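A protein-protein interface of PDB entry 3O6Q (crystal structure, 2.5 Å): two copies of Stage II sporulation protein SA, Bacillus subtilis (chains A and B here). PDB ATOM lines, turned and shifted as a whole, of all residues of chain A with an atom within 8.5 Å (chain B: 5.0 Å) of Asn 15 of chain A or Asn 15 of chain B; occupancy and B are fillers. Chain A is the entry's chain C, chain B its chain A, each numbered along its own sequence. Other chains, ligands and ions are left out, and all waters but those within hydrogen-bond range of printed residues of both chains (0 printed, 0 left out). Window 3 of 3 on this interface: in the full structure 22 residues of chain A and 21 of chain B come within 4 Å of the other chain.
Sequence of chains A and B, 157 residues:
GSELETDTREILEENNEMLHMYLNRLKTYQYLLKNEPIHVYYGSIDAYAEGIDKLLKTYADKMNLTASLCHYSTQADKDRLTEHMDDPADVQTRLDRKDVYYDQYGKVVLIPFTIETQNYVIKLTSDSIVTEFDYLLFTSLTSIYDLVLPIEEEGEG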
ATOM      1  N   THR A   8     -17.729  16.475 -30.176  1.00  0.00           N
ATOM      2  CA  THR A   8     -18.221  15.781 -28.986  1.00  0.00           C
ATOM      3  C   THR A   8     -18.366  16.769 -27.814  1.00  0.00           C
ATOM      4  O   THR A   8     -19.166  16.539 -26.911  1.00  0.00           O
ATOM      5  CB  THR A   8     -17.286  14.598 -28.594  1.00  0.00           C
ATOM      6  OG1 THR A   8     -16.031  15.097 -28.117  1.00  0.00           O
ATOM      7  CG2 THR A   8     -17.037  13.674 -29.788  1.00  0.00           C
ATOM      8  N   ARG A   9     -17.588  17.854 -27.845  1.00  0.00           N
ATOM      9  CA  ARG A   9     -17.722  18.966 -26.884  1.00  0.00           C
ATOM     10  C   ARG A   9     -19.155  19.499 -26.791  1.00  0.00           C
ATOM     11  O   ARG A   9     -19.719  19.595 -25.695  1.00  0.00           O
ATOM     12  CB  ARG A   9     -16.744  20.105 -27.229  1.00  0.00           C
ATOM     13  CG  ARG A   9     -17.260  21.526 -26.963  1.00  0.00           C
ATOM     14  CD  ARG A   9     -16.401  22.367 -26.016  1.00  0.00           C
ATOM     15  NE  ARG A   9     -17.035  23.657 -25.721  1.00  0.00           N
ATOM     16  CZ  ARG A   9     -17.137  24.682 -26.573  1.00  0.00           C
ATOM     17  NH1 ARG A   9     -16.641  24.610 -27.807  1.00  0.00           N
ATOM     18  NH2 ARG A   9     -17.745  25.801 -26.193  1.00  0.00           N
ATOM     19  N   GLU A  10     -19.734  19.867 -27.927  1.00  0.00           N
ATOM     20  CA  GLU A  10     -21.096  20.390 -27.930  1.00  0.00           C
ATOM     21  C   GLU A  10     -22.077  19.392 -27.356  1.00  0.00           C
ATOM     22  O   GLU A  10     -22.853  19.736 -26.476  1.00  0.00           O
ATOM     23  CB  GLU A  10     -21.518  20.797 -29.343  1.00  0.00           C
ATOM     24  CG  GLU A  10     -20.876  22.105 -29.816  1.00  0.00           C
ATOM     25  CD  GLU A  10     -21.226  23.292 -28.921  1.00  0.00           C
ATOM     26  OE1 GLU A  10     -22.334  23.286 -28.319  1.00  0.00           O
ATOM     27  OE2 GLU A  10     -20.389  24.222 -28.817  1.00  0.00           O
ATOM     28  N   ILE A  11     -22.028  18.155 -27.844  1.00  0.00           N
ATOM     29  CA  ILE A  11     -22.921  17.080 -27.367  1.00  0.00           C
ATOM     30  C   ILE A  11     -22.834  16.893 -25.866  1.00  0.00           C
ATOM     31  O   ILE A  11     -23.808  16.612 -25.183  1.00  0.00           O
ATOM     32  CB  ILE A  11     -22.544  15.728 -27.993  1.00  0.00           C
ATOM     33  CG1 ILE A  11     -22.788  15.742 -29.498  1.00  0.00           C
ATOM     34  CG2 ILE A  11     -23.352  14.633 -27.398  1.00  0.00           C
ATOM     35  CD1 ILE A  11     -21.588  16.198 -30.376  1.00  0.00           C
ATOM     36  N   LEU A  12     -21.622  17.041 -25.368  1.00  0.00           N
ATOM     37  CA  LEU A  12     -21.321  16.882 -23.950  1.00  0.00           C
ATOM     38  C   LEU A  12     -21.946  17.987 -23.103  1.00  0.00           C
ATOM     39  O   LEU A  12     -22.480  17.726 -22.039  1.00  0.00           O
ATOM     40  CB  LEU A  12     -19.797  16.897 -23.794  1.00  0.00           C
ATOM     41  CG  LEU A  12     -19.182  15.938 -22.781  1.00  0.00           C
ATOM     42  CD1 LEU A  12     -19.991  14.631 -22.591  1.00  0.00           C
ATOM     43  CD2 LEU A  12     -17.785  15.653 -23.249  1.00  0.00           C
ATOM     44  N   GLU A  13     -21.851  19.223 -23.577  1.00  0.00           N
ATOM     45  CA  GLU A  13     -22.508  20.364 -22.948  1.00  0.00           C
ATOM     46  C   GLU A  13     -24.024  20.163 -22.977  1.00  0.00           C
ATOM     47  O   GLU A  13     -24.720  20.499 -22.004  1.00  0.00           O
ATOM     48  CB  GLU A  13     -22.128  21.678 -23.668  1.00  0.00           C
ATOM     49  CG  GLU A  13     -21.103  22.580 -22.967  1.00  0.00           C
ATOM     50  CD  GLU A  13     -20.399  23.574 -23.952  1.00  0.00           C
ATOM     51  OE1 GLU A  13     -21.002  23.942 -24.989  1.00  0.00           O
ATOM     52  OE2 GLU A  13     -19.243  23.988 -23.694  1.00  0.00           O
ATOM     53  N   GLU A  14     -24.541  19.597 -24.072  1.00  0.00           N
ATOM     54  CA  GLU A  14     -25.978  19.306 -24.157  1.00  0.00           C
ATOM     55  C   GLU A  14     -26.395  18.241 -23.140  1.00  0.00           C
ATOM     56  O   GLU A  14     -27.424  18.384 -22.462  1.00  0.00           O
ATOM     57  CB  GLU A  14     -26.367  18.877 -25.578  1.00  0.00           C
ATOM     58  CG  GLU A  14     -26.411  20.036 -26.596  1.00  0.00           C
ATOM     59  CD  GLU A  14     -27.323  19.777 -27.803  1.00  0.00           C
ATOM     60  OE1 GLU A  14     -28.505  19.399 -27.588  1.00  0.00           O
ATOM     61  OE2 GLU A  14     -26.860  19.956 -28.963  1.00  0.00           O
ATOM     62  N   ASN A  15     -25.611  17.169 -23.036  1.00  0.00           N
ATOM     63  CA  ASN A  15     -25.892  16.119 -22.055  1.00  0.00           C
ATOM     64  C   ASN A  15     -25.848  16.699 -20.645  1.00  0.00           C
ATOM     65  O   ASN A  15     -26.744  16.460 -19.825  1.00  0.00           O
ATOM     66  CB  ASN A  15     -24.894  14.962 -22.185  1.00  0.00           C
ATOM     67  CG  ASN A  15     -25.172  14.071 -23.398  1.00  0.00           C
ATOM     68  OD1 ASN A  15     -24.749  14.388 -24.494  1.00  0.00           O
ATOM     69  ND2 ASN A  15     -25.862  12.949 -23.195  1.00  0.00           N
ATOM     70  N   ASN A  16     -24.814  17.488 -20.386  1.00  0.00           N
ATOM     71  CA  ASN A  16     -24.604  18.051 -19.075  1.00  0.00           C
ATOM     72  C   ASN A  16     -25.718  18.984 -18.682  1.00  0.00           C
ATOM     73  O   ASN A  16     -26.208  18.941 -17.558  1.00  0.00           O
ATOM     74  CB  ASN A  16     -23.261  18.793 -19.016  1.00  0.00           C
ATOM     75  CG  ASN A  16     -22.848  19.106 -17.596  1.00  0.00           C
ATOM     76  OD1 ASN A  16     -23.125  18.332 -16.660  1.00  0.00           O
ATOM     77  ND2 ASN A  16     -22.210  20.233 -17.411  1.00  0.00           N
ATOM     78  N   GLU A  17     -26.110  19.836 -19.623  1.00  0.00           N
ATOM     79  CA  GLU A  17     -27.225  20.758 -19.421  1.00  0.00           C
ATOM     80  C   GLU A  17     -28.499  19.996 -19.119  1.00  0.00           C
ATOM     81  O   GLU A  17     -29.177  20.315 -18.152  1.00  0.00           O
ATOM     82  CB  GLU A  17     -27.386  21.666 -20.650  1.00  0.00           C
ATOM     83  CG  GLU A  17     -28.704  22.476 -20.729  1.00  0.00           C
ATOM     84  CD  GLU A  17     -29.336  22.528 -22.135  1.00  0.00           C
ATOM     85  OE1 GLU A  17     -30.040  21.547 -22.505  1.00  0.00           O
ATOM     86  OE2 GLU A  17     -29.176  23.557 -22.842  1.00  0.00           O
ATOM     87  N   MET A  18     -28.815  18.981 -19.926  1.00  0.00           N
ATOM     88  CA  MET A  18     -30.001  18.142 -19.707  1.00  0.00           C
ATOM     89  C   MET A  18     -30.051  17.552 -18.296  1.00  0.00           C
ATOM     90  O   MET A  18     -31.097  17.519 -17.668  1.00  0.00           O
ATOM     91  CB  MET A  18     -30.012  16.974 -20.687  1.00  0.00           C
ATOM     92  CG  MET A  18     -30.359  17.326 -22.135  1.00  0.00           C
ATOM     93  SD  MET A  18     -32.298  17.262 -22.479  1.00  0.00           S
ATOM     94  CE  MET A  18     -32.302  15.319 -22.739  1.00  0.00           C
ATOM     95  N   LEU A  19     -28.912  17.071 -17.806  1.00  0.00           N
ATOM     96  CA  LEU A  19     -28.891  16.387 -16.523  1.00  0.00           C
ATOM     97  C   LEU A  19     -29.045  17.333 -15.373  1.00  0.00           C
ATOM     98  O   LEU A  19     -29.686  17.000 -14.390  1.00  0.00           O
ATOM     99  CB  LEU A  19     -27.589  15.605 -16.320  1.00  0.00           C
ATOM    100  CG  LEU A  19     -27.551  14.263 -17.003  1.00  0.00           C
ATOM    101  CD1 LEU A  19     -26.160  13.726 -16.725  1.00  0.00           C
ATOM    102  CD2 LEU A  19     -28.632  13.343 -16.440  1.00  0.00           C
ATOM    103  N   HIS A  20     -28.402  18.486 -15.481  1.00  0.00           N
ATOM    104  CA  HIS A  20     -28.536  19.515 -14.475  1.00  0.00           C
ATOM    105  C   HIS A  20     -29.945  20.031 -14.438  1.00  0.00           C
ATOM    106  O   HIS A  20     -30.574  20.069 -13.374  1.00  0.00           O
ATOM    107  CB  HIS A  20     -27.586  20.653 -14.741  1.00  0.00           C
ATOM    108  CG  HIS A  20     -26.316  20.518 -13.981  1.00  0.00           C
ATOM    109  ND1 HIS A  20     -25.137  20.120 -14.567  1.00  0.00           N
ATOM    110  CD2 HIS A  20     -26.063  20.635 -12.656  1.00  0.00           C
ATOM    111  CE1 HIS A  20     -24.200  20.050 -13.643  1.00  0.00           C
ATOM    112  NE2 HIS A  20     -24.739  20.349 -12.476  1.00  0.00           N
ATOM    113  N   MET A  21     -30.442  20.401 -15.608  1.00  0.00           N
ATOM    114  CA  MET A  21     -31.742  21.026 -15.675  1.00  0.00           C
ATOM    115  C   MET A  21     -32.832  20.123 -15.111  1.00  0.00           C
ATOM    116  O   MET A  21     -33.650  20.598 -14.323  1.00  0.00           O
ATOM    117  CB  MET A  21     -32.070  21.427 -17.099  1.00  0.00           C
ATOM    118  CG  MET A  21     -33.255  22.413 -17.192  1.00  0.00           C
ATOM    119  SD  MET A  21     -32.785  24.328 -16.818  1.00  0.00           S
ATOM    120  CE  MET A  21     -32.368  24.221 -14.901  1.00  0.00           C
ATOM    121  N   TYR A  22     -32.830  18.844 -15.470  1.00  0.00           N
ATOM    122  CA  TYR A  22     -33.867  17.979 -15.022  1.00  0.00           C
ATOM    123  C   TYR A  22     -33.674  17.395 -13.634  1.00  0.00           C
ATOM    124  O   TYR A  22     -34.635  17.104 -12.941  1.00  0.00           O
ATOM    125  CB  TYR A  22     -34.167  16.966 -16.108  1.00  0.00           C
ATOM    126  CG  TYR A  22     -34.817  17.711 -17.286  1.00  0.00           C
ATOM    127  CD1 TYR A  22     -36.040  18.395 -17.117  1.00  0.00           C
ATOM    128  CD2 TYR A  22     -34.197  17.798 -18.529  1.00  0.00           C
ATOM    129  CE1 TYR A  22     -36.636  19.109 -18.156  1.00  0.00           C
ATOM    130  CE2 TYR A  22     -34.786  18.533 -19.582  1.00  0.00           C
ATOM    131  CZ  TYR A  22     -36.008  19.178 -19.378  1.00  0.00           C
ATOM    132  OH  TYR A  22     -36.604  19.890 -20.386  1.00  0.00           O
ATOM    133  N   ILE B  11     -17.494   8.500 -20.355  1.00  0.00           N
ATOM    134  CA  ILE B  11     -18.347   9.520 -19.751  1.00  0.00           C
ATOM    135  C   ILE B  11     -19.606   9.785 -20.600  1.00  0.00           C
ATOM    136  O   ILE B  11     -20.659  10.102 -20.070  1.00  0.00           O
ATOM    137  CB  ILE B  11     -17.626  10.860 -19.550  1.00  0.00           C
ATOM    138  CG1 ILE B  11     -18.523  11.808 -18.730  1.00  0.00           C
ATOM    139  CG2 ILE B  11     -17.296  11.470 -20.884  1.00  0.00           C
ATOM    140  CD1 ILE B  11     -17.902  13.097 -18.356  1.00  0.00           C
ATOM    141  N   LEU B  12     -19.461   9.668 -21.912  1.00  0.00           N
ATOM    142  CA  LEU B  12     -20.543   9.861 -22.858  1.00  0.00           C
ATOM    143  C   LEU B  12     -21.595   8.758 -22.721  1.00  0.00           C
ATOM    144  O   LEU B  12     -22.800   9.036 -22.723  1.00  0.00           O
ATOM    145  CB  LEU B  12     -19.949   9.846 -24.260  1.00  0.00           C
ATOM    146  CG  LEU B  12     -20.455  10.738 -25.370  1.00  0.00           C
ATOM    147  CD1 LEU B  12     -20.560  12.159 -24.855  1.00  0.00           C
ATOM    148  CD2 LEU B  12     -19.484  10.633 -26.531  1.00  0.00           C
ATOM    149  N   GLU B  13     -21.134   7.516 -22.594  1.00  0.00           N
ATOM    150  CA  GLU B  13     -22.005   6.381 -22.314  1.00  0.00           C
ATOM    151  C   GLU B  13     -22.680   6.562 -20.956  1.00  0.00           C
ATOM    152  O   GLU B  13     -23.852   6.207 -20.781  1.00  0.00           O
ATOM    153  CB  GLU B  13     -21.228   5.051 -22.364  1.00  0.00           C
ATOM    154  CG  GLU B  13     -21.459   4.235 -23.658  1.00  0.00           C
ATOM    155  CD  GLU B  13     -20.275   3.370 -24.080  1.00  0.00           C
ATOM    156  OE1 GLU B  13     -19.186   3.936 -24.307  1.00  0.00           O
ATOM    157  OE2 GLU B  13     -20.428   2.131 -24.220  1.00  0.00           O
ATOM    158  N   GLU B  14     -21.954   7.119 -19.991  1.00  0.00           N
ATOM    159  CA  GLU B  14     -22.547   7.356 -18.662  1.00  0.00           C
ATOM    160  C   GLU B  14     -23.632   8.426 -18.730  1.00  0.00           C
ATOM    161  O   GLU B  14     -24.678   8.259 -18.143  1.00  0.00           O
ATOM    162  CB  GLU B  14     -21.497   7.764 -17.632  1.00  0.00           C
ATOM    163  CG  GLU B  14     -21.622   7.049 -16.288  1.00  0.00           C
ATOM    164  CD  GLU B  14     -20.298   6.973 -15.554  1.00  0.00           C
ATOM    165  OE1 GLU B  14     -19.361   7.733 -15.902  1.00  0.00           O
ATOM    166  OE2 GLU B  14     -20.187   6.138 -14.630  1.00  0.00           O
ATOM    167  N   ASN B  15     -23.382   9.519 -19.455  1.00  0.00           N
ATOM    168  CA  ASN B  15     -24.412  10.575 -19.656  1.00  0.00           C
ATOM    169  C   ASN B  15     -25.622   9.997 -20.365  1.00  0.00           C
ATOM    170  O   ASN B  15     -26.737  10.150 -19.913  1.00  0.00           O
ATOM    171  CB  ASN B  15     -23.864  11.754 -20.461  1.00  0.00           C
ATOM    172  CG  ASN B  15     -23.092  12.737 -19.596  1.00  0.00           C
ATOM    173  OD1 ASN B  15     -21.917  13.016 -19.844  1.00  0.00           O
ATOM    174  ND2 ASN B  15     -23.740  13.226 -18.542  1.00  0.00           N
ATOM    175  N   ASN B  16     -25.363   9.256 -21.437  1.00  0.00           N
ATOM    176  CA  ASN B  16     -26.405   8.651 -22.224  1.00  0.00           C
ATOM    177  C   ASN B  16     -27.268   7.678 -21.415  1.00  0.00           C
ATOM    178  O   ASN B  16     -28.490   7.736 -21.479  1.00  0.00           O
ATOM    179  CB  ASN B  16     -25.788   7.934 -23.422  1.00  0.00           C
ATOM    180  CG  ASN B  16     -26.782   7.667 -24.496  1.00  0.00           C
ATOM    181  OD1 ASN B  16     -27.528   8.560 -24.878  1.00  0.00           O
ATOM    182  ND2 ASN B  16     -26.821   6.438 -24.990  1.00  0.00           N
ATOM    183  N   GLU B  17     -26.615   6.808 -20.655  1.00  0.00           N
ATOM    184  CA  GLU B  17     -27.287   5.880 -19.766  1.00  0.00           C
ATOM    185  C   GLU B  17     -28.142   6.618 -18.744  1.00  0.00           C
ATOM    186  O   GLU B  17     -29.313   6.293 -18.588  1.00  0.00           O
ATOM    187  CB  GLU B  17     -26.273   4.973 -19.085  1.00  0.00           C
ATOM    188  CG  GLU B  17     -26.782   4.171 -17.871  1.00  0.00           C
ATOM    189  CD  GLU B  17     -25.735   4.170 -16.746  1.00  0.00           C
ATOM    190  OE1 GLU B  17     -24.920   3.223 -16.696  1.00  0.00           O
ATOM    191  OE2 GLU B  17     -25.687   5.150 -15.952  1.00  0.00           O
ATOM    192  N   MET B  18     -27.580   7.617 -18.070  1.00  0.00           N
ATOM    193  CA  MET B  18     -28.331   8.433 -17.100  1.00  0.00           C
ATOM    194  C   MET B  18     -29.610   9.030 -17.707  1.00  0.00           C
ATOM    195  O   MET B  18     -30.661   9.033 -17.065  1.00  0.00           O
ATOM    196  CB  MET B  18     -27.468   9.597 -16.606  1.00  0.00           C
ATOM    197  CG  MET B  18     -26.321   9.226 -15.669  1.00  0.00           C
ATOM    198  SD  MET B  18     -26.937   9.013 -13.834  1.00  0.00           S
ATOM    199  CE  MET B  18     -27.433  10.830 -13.329  1.00  0.00           C
ATOM    200  N   LEU B  19     -29.508   9.580 -18.915  1.00  0.00           N
ATOM    201  CA  LEU B  19     -30.637  10.300 -19.503  1.00  0.00           C
ATOM    202  C   LEU B  19     -31.731   9.347 -19.940  1.00  0.00           C
ATOM    203  O   LEU B  19     -32.910   9.643 -19.780  1.00  0.00           O
ATOM    204  CB  LEU B  19     -30.202  11.121 -20.710  1.00  0.00           C
ATOM    205  CG  LEU B  19     -29.466  12.449 -20.422  1.00  0.00           C
ATOM    206  CD1 LEU B  19     -28.674  12.965 -21.641  1.00  0.00           C
ATOM    207  CD2 LEU B  19     -30.452  13.513 -19.853  1.00  0.00           C
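Among the printed residues, merely in contact across the chains: Leu 19 of chain A with Asn 15 of chain B (3.1 Å), Asn 15 of chain A with Leu 19 of chain B (3.2 Å), Leu 12 of chain A with Leu 12 of chain B (3.4 Å), Met 18 of chain A with Leu 19 of chain B (3.6 Å), Asn 15 of chain A with Asn 15 of chain B (3.6 Å), Leu 12 of chain A with Asn 15 of chain B (3.7 Å), Leu 19 of chain A with Leu 19 of chain B (3.9 Å) and Leu 19 of chain A with Met 18 of chain B (3.9 Å).
The backbone carbonyl oxygen (O) of Ile 11 of chain B lies close to the side-chain amide oxygen (OD1) of Asn 15 of chain B (3.2 Å).
O of Ile 11 of chain A sits close to OD1 of Asn 15 of chain A.
Leu 12 of chain A touches Asn 15 of chain B, but with the chains exchanged Asn 15 of chain A does not touch Leu 12 of chain B (4.8 Å).
Asn 15 of chain A touches Leu 19 of chain B, and with the chains exchanged Leu 19 of chain A touches Asn 15 of chain B.
Met 18 of chain A touches Leu 19 of chain B, and with the chains exchanged Leu 19 of chain A touches Met 18 of chain B.
Leu 19 of chain B touches its own counterpart, Leu 19 of chain A.
Of the 8 pairs that touch across the chains among the printed residues, 7 have their exchanged pair printed and touching as well.
Asn 15 of chain A touches just these residues of chain B: Asn 15 (3.6 Å) and Leu 19 (3.2 Å).
Asn 15 of chain B touches three residues of chain A.
Printed residues of chain A within 4 Å of Leu 19 of chain B: Asn 15, Met 18 and Leu 19.
Printed residues of chain A within 4 Å of Leu 12 of chain B: Leu 12.
Of the printed residues of chain A, Met 18 of chain B touches Leu 19 (3.9 Å).
Printed residues of chain B within 4 Å of Leu 19 of chain A: Asn 15 (3.1 Å), Met 18 (3.9 Å) and Leu 19 (3.9 Å).
Of the 9 printed residues of chain B, 4 touch a printed residue of chain A.
Hydrophobic or aromatic side chains of chain B that line the printed part of chain A: Leu 12, Met 18 and Leu 19.
Hydrophobic or aromatic side chains of chain A within 4 Å of the printed part of chain B: Leu 12, Met 18 and Leu 19.
Among the printed residues, 8 pairs touch across the chains.
Among the printed residues, no Asp or Glu carboxylate lies within 4 Å of a Lys or Arg side-chain nitrogen of the other chain.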
